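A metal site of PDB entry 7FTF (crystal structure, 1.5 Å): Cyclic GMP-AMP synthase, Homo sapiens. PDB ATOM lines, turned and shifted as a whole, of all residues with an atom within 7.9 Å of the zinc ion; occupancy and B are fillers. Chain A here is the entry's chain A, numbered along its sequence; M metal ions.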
ATOM      1  N   LEU A 227      17.157  20.885 -19.396  1.00  0.00           N
ATOM      2  CA  LEU A 227      17.309  22.214 -19.964  1.00  0.00           C
ATOM      3  C   LEU A 227      16.515  22.374 -21.251  1.00  0.00           C
ATOM      4  O   LEU A 227      16.018  23.471 -21.536  1.00  0.00           O
ATOM      5  CB  LEU A 227      18.776  22.543 -20.238  1.00  0.00           C
ATOM      6  CG  LEU A 227      19.436  23.550 -19.298  1.00  0.00           C
ATOM      7  CD1 LEU A 227      20.920  23.646 -19.605  1.00  0.00           C
ATOM      8  CD2 LEU A 227      18.761  24.922 -19.392  1.00  0.00           C
ATOM      9  N   ASN A 228      16.388  21.296 -22.026  1.00  0.00           N
ATOM     10  CA  ASN A 228      15.670  21.295 -23.294  1.00  0.00           C
ATOM     11  C   ASN A 228      14.185  21.010 -23.148  1.00  0.00           C
ATOM     12  O   ASN A 228      13.435  21.248 -24.097  1.00  0.00           O
ATOM     13  CB  ASN A 228      16.276  20.270 -24.244  1.00  0.00           C
ATOM     14  CG  ASN A 228      17.597  20.728 -24.825  1.00  0.00           C
ATOM     15  OD1 ASN A 228      17.897  21.914 -24.833  1.00  0.00           O
ATOM     16  ND2 ASN A 228      18.385  19.777 -25.324  1.00  0.00           N
ATOM     17  N   ASN A 229      13.759  20.437 -22.041  1.00  0.00           N
ATOM     18  CA  ASN A 229      12.357  20.133 -21.800  1.00  0.00           C
ATOM     19  C   ASN A 229      12.033  20.683 -20.407  1.00  0.00           C
ATOM     20  O   ASN A 229      11.924  19.962 -19.413  1.00  0.00           O
ATOM     21  CB  ASN A 229      12.112  18.629 -21.926  1.00  0.00           C
ATOM     22  CG  ASN A 229      10.647  18.265 -21.893  1.00  0.00           C
ATOM     23  OD1 ASN A 229       9.763  19.113 -21.802  1.00  0.00           O
ATOM     24  ND2 ASN A 229      10.382  16.957 -21.987  1.00  0.00           N
ATOM     25  N   HIS A 230      11.970  22.017 -20.317  1.00  0.00           N
ATOM     26  CA  HIS A 230      12.226  22.738 -19.082  1.00  0.00           C
ATOM     27  C   HIS A 230      10.999  23.387 -18.466  1.00  0.00           C
ATOM     28  O   HIS A 230      11.136  24.077 -17.455  1.00  0.00           O
ATOM     29  CB  HIS A 230      13.248  23.847 -19.353  1.00  0.00           C
ATOM     30  CG  HIS A 230      12.786  24.809 -20.419  1.00  0.00           C
ATOM     31  ND1 HIS A 230      13.447  24.962 -21.621  1.00  0.00           N
ATOM     32  CD2 HIS A 230      11.672  25.581 -20.502  1.00  0.00           C
ATOM     33  CE1 HIS A 230      12.780  25.830 -22.379  1.00  0.00           C
ATOM     34  NE2 HIS A 230      11.698  26.210 -21.720  1.00  0.00           N
ATOM     35  N   GLY A 231       9.835  23.248 -19.076  1.00  0.00           N
ATOM     36  CA  GLY A 231       8.665  23.952 -18.585  1.00  0.00           C
ATOM     37  C   GLY A 231       7.792  23.104 -17.688  1.00  0.00           C
ATOM     38  O   GLY A 231       7.810  21.870 -17.755  1.00  0.00           O
ATOM     39  N   LYS A 232       6.978  23.779 -16.862  1.00  0.00           N
ATOM     40  CA  LYS A 232       5.848  23.053 -16.274  1.00  0.00           C
ATOM     41  C   LYS A 232       4.886  22.616 -17.364  1.00  0.00           C
ATOM     42  O   LYS A 232       4.398  21.483 -17.362  1.00  0.00           O
ATOM     43  CB  LYS A 232       5.122  23.897 -15.234  1.00  0.00           C
ATOM     44  CG  LYS A 232       3.912  23.133 -14.690  1.00  0.00           C
ATOM     45  CD  LYS A 232       3.287  23.850 -13.515  1.00  0.00           C
ATOM     46  CE  LYS A 232       4.203  23.804 -12.291  1.00  0.00           C
ATOM     47  NZ  LYS A 232       4.589  22.398 -11.903  1.00  0.00           N
ATOM     48  N   SER A 233       4.587  23.527 -18.299  1.00  0.00           N
ATOM     49  CA  SER A 233       3.817  23.147 -19.481  1.00  0.00           C
ATOM     50  C   SER A 233       4.649  22.283 -20.418  1.00  0.00           C
ATOM     51  O   SER A 233       5.787  22.647 -20.736  1.00  0.00           O
ATOM     52  CB  SER A 233       3.388  24.375 -20.274  1.00  0.00           C
ATOM     53  OG  SER A 233       2.747  23.950 -21.483  1.00  0.00           O
ATOM     54  N   THR A 235       4.242  22.175 -23.496  1.00  0.00           N
ATOM     55  CA  THR A 235       4.458  22.957 -24.710  1.00  0.00           C
ATOM     56  C   THR A 235       5.204  24.268 -24.442  1.00  0.00           C
ATOM     57  O   THR A 235       5.212  25.149 -25.316  1.00  0.00           O
ATOM     58  CB  THR A 235       3.120  23.207 -25.436  1.00  0.00           C
ATOM     59  OG1 THR A 235       2.126  23.645 -24.495  1.00  0.00           O
ATOM     60  CG2 THR A 235       2.613  21.916 -26.060  1.00  0.00           C
ATOM     61  N   CYS A 236       5.875  24.400 -23.288  1.00  0.00           N
ATOM     62  CA  CYS A 236       6.719  25.570 -23.076  1.00  0.00           C
ATOM     63  C   CYS A 236       7.701  25.738 -24.215  1.00  0.00           C
ATOM     64  O   CYS A 236       8.364  24.774 -24.635  1.00  0.00           O
ATOM     65  CB  CYS A 236       7.472  25.456 -21.742  1.00  0.00           C
ATOM     66  SG  CYS A 236       8.240  27.032 -21.179  1.00  0.00           S
ATOM     67  N   CYS A 237       7.748  26.950 -24.772  1.00  0.00           N
ATOM     68  CA  CYS A 237       8.607  27.349 -25.884  1.00  0.00           C
ATOM     69  C   CYS A 237       8.313  26.609 -27.187  1.00  0.00           C
ATOM     70  O   CYS A 237       9.072  26.744 -28.163  1.00  0.00           O
ATOM     71  CB  CYS A 237      10.111  27.224 -25.494  1.00  0.00           C
ATOM     72  SG  CYS A 237      10.599  28.457 -24.238  1.00  0.00           S
ATOM     73  N   GLU A 238       7.169  25.926 -27.294  1.00  0.00           N
ATOM     74  CA  GLU A 238       6.781  25.325 -28.570  1.00  0.00           C
ATOM     75  C   GLU A 238       5.817  26.191 -29.389  1.00  0.00           C
ATOM     76  O   GLU A 238       5.454  25.808 -30.506  1.00  0.00           O
ATOM     77  CB  GLU A 238       6.144  23.936 -28.343  1.00  0.00           C
ATOM     78  CG  GLU A 238       7.163  22.876 -27.913  1.00  0.00           C
ATOM     79  CD  GLU A 238       6.666  21.435 -28.099  1.00  0.00           C
ATOM     80  OE1 GLU A 238       5.473  21.223 -28.392  1.00  0.00           O
ATOM     81  OE2 GLU A 238       7.495  20.513 -27.931  1.00  0.00           O
ATOM     82  N   GLU A 242       3.852  30.746 -25.346  1.00  0.00           N
ATOM     83  CA  GLU A 242       4.570  30.134 -24.223  1.00  0.00           C
ATOM     84  C   GLU A 242       6.082  30.304 -24.375  1.00  0.00           C
ATOM     85  O   GLU A 242       6.864  29.364 -24.202  1.00  0.00           O
ATOM     86  CB  GLU A 242       4.214  28.654 -24.094  1.00  0.00           C
ATOM     87  CG  GLU A 242       2.747  28.409 -23.816  1.00  0.00           C
ATOM     88  CD  GLU A 242       2.469  26.918 -23.590  1.00  0.00           C
ATOM     89  OE1 GLU A 242       2.926  26.415 -22.546  1.00  0.00           O
ATOM     90  OE2 GLU A 242       1.818  26.267 -24.445  1.00  0.00           O
ATOM     91  N   LYS A 243       6.537  31.500 -24.616  1.00  0.00           N
ATOM     92  CA  LYS A 243       7.973  31.745 -24.777  1.00  0.00           C
ATOM     93  C   LYS A 243       8.509  32.176 -23.420  1.00  0.00           C
ATOM     94  O   LYS A 243       8.298  33.314 -23.002  1.00  0.00           O
ATOM     95  CB  LYS A 243       8.218  32.801 -25.861  1.00  0.00           C
ATOM     96  CG  LYS A 243       8.027  32.294 -27.308  1.00  0.00           C
ATOM     97  CD  LYS A 243       8.712  30.948 -27.492  1.00  0.00           C
ATOM     98  CE  LYS A 243       9.163  30.677 -28.915  1.00  0.00           C
ATOM     99  NZ  LYS A 243      10.121  29.517 -28.921  1.00  0.00           N
ATOM    100  N   CYS A 244       9.206  31.282 -22.719  1.00  0.00           N
ATOM    101  CA  CYS A 244       9.766  31.675 -21.437  1.00  0.00           C
ATOM    102  C   CYS A 244      11.217  32.131 -21.585  1.00  0.00           C
ATOM    103  O   CYS A 244      11.796  32.046 -22.661  1.00  0.00           O
ATOM    104  CB  CYS A 244       9.663  30.521 -20.429  1.00  0.00           C
ATOM    105  SG  CYS A 244      11.003  29.263 -20.588  1.00  0.00           S
ATOM    106  N   CYS A 245      11.785  32.662 -20.502  1.00  0.00           N
ATOM    107  CA  CYS A 245      13.138  33.186 -20.589  1.00  0.00           C
ATOM    108  C   CYS A 245      14.139  32.369 -19.774  1.00  0.00           C
ATOM    109  O   CYS A 245      15.199  32.876 -19.410  1.00  0.00           O
ATOM    110  CB  CYS A 245      13.210  34.652 -20.157  1.00  0.00           C
ATOM    111  SG  CYS A 245      12.835  34.931 -18.378  1.00  0.00           S
ATOM    112  N   ARG A 246      13.846  31.085 -19.549  1.00  0.00           N
ATOM    113  CA  ARG A 246      14.754  30.261 -18.749  1.00  0.00           C
ATOM    114  C   ARG A 246      16.112  30.117 -19.430  1.00  0.00           C
ATOM    115  O   ARG A 246      17.162  30.360 -18.794  1.00  0.00           O
ATOM    116  CB  ARG A 246      14.136  28.875 -18.485  1.00  0.00           C
ATOM    117  CG  ARG A 246      13.064  28.860 -17.417  1.00  0.00           C
ATOM    118  CD  ARG A 246      12.584  27.411 -17.236  1.00  0.00           C
ATOM    119  NE  ARG A 246      11.512  27.207 -16.278  1.00  0.00           N
ATOM    120  CZ  ARG A 246      10.217  27.216 -16.597  1.00  0.00           C
ATOM    121  NH1 ARG A 246       9.321  26.938 -15.630  1.00  0.00           N
ATOM    122  NH2 ARG A 246       9.820  27.508 -17.858  1.00  0.00           N
ATOM    123  N   LYS A 247      16.119  29.729 -20.713  1.00  0.00           N
ATOM    124  CA  LYS A 247      17.403  29.512 -21.381  1.00  0.00           C
ATOM    125  C   LYS A 247      18.194  30.810 -21.487  1.00  0.00           C
ATOM    126  O   LYS A 247      19.422  30.814 -21.288  1.00  0.00           O
ATOM    127  CB  LYS A 247      17.213  28.891 -22.760  1.00  0.00           C
ATOM    128  CG  LYS A 247      16.955  27.357 -22.697  1.00  0.00           C
ATOM    129  CD  LYS A 247      17.034  26.788 -24.097  1.00  0.00           C
ATOM    130  CE  LYS A 247      16.844  25.286 -24.136  1.00  0.00           C
ATOM    131  NZ  LYS A 247      16.944  24.777 -25.530  1.00  0.00           N
ATOM    132  N   ASP A 292       5.732  28.442 -15.159  1.00  0.00           N
ATOM    133  CA  ASP A 292       6.203  29.126 -16.357  1.00  0.00           C
ATOM    134  C   ASP A 292       5.900  30.622 -16.311  1.00  0.00           C
ATOM    135  O   ASP A 292       6.624  31.425 -16.917  1.00  0.00           O
ATOM    136  CB  ASP A 292       5.576  28.506 -17.619  1.00  0.00           C
ATOM    137  CG  ASP A 292       5.951  27.030 -17.807  1.00  0.00           C
ATOM    138  OD1 ASP A 292       6.980  26.572 -17.263  1.00  0.00           O
ATOM    139  OD2 ASP A 292       5.187  26.330 -18.504  1.00  0.00           O
ATOM    140  N   TRP A 295       8.685  32.950 -15.421  1.00  0.00           N
ATOM    141  CA  TRP A 295       9.748  33.037 -16.420  1.00  0.00           C
ATOM    142  C   TRP A 295       9.217  33.669 -17.687  1.00  0.00           C
ATOM    143  O   TRP A 295       9.664  33.367 -18.797  1.00  0.00           O
ATOM    144  CB  TRP A 295      10.345  31.651 -16.707  1.00  0.00           C
ATOM    145  CG  TRP A 295      10.968  31.028 -15.490  1.00  0.00           C
ATOM    146  CD1 TRP A 295      10.372  30.173 -14.593  1.00  0.00           C
ATOM    147  CD2 TRP A 295      12.311  31.231 -15.028  1.00  0.00           C
ATOM    148  NE1 TRP A 295      11.266  29.835 -13.604  1.00  0.00           N
ATOM    149  CE2 TRP A 295      12.464  30.460 -13.854  1.00  0.00           C
ATOM    150  CE3 TRP A 295      13.400  31.987 -15.500  1.00  0.00           C
ATOM    151  CZ2 TRP A 295      13.671  30.407 -13.138  1.00  0.00           C
ATOM    152  CZ3 TRP A 295      14.607  31.948 -14.787  1.00  0.00           C
ATOM    153  CH2 TRP A 295      14.726  31.166 -13.608  1.00  0.00           C
HETATM  154 ZN    ZN M   1      10.216  27.608 -22.150  1.00  0.00          ZN
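The backbone carbonyl oxygen of His 230 sits at hydrogen-bond distance from the guanidinium group of Arg 246, 3.4 Å away.
O of Leu 227 lies within hydrogen-bond range of ND1 of His 230.
SG of Cys 236 lies close to NH2 of Arg 246.
O of Glu 242 lies within hydrogen-bond range of N of Cys 237 (2.6 Å).
The backbone carbonyl oxygen (O) of Cys 237 sits at hydrogen-bond distance from the side-chain amino group (NZ) of Lys 243 (3.1 Å).
The side-chain sulfur (SG) of Cys 244 lies close to the guanidinium group (NH2) of Arg 246, at 3.5 Å.
The zinc ion is bound by NE2 of His 230 (2.1 Å), SG of Cys 236 (2.3 Å), SG of Cys 237 (2.3 Å) and SG of Cys 244 (2.4 Å).
The zinc ion has four donor atoms within binding distance.
Within 4 Å of the zinc ion: His 230, Cys 236, Cys 237 and Cys 244.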
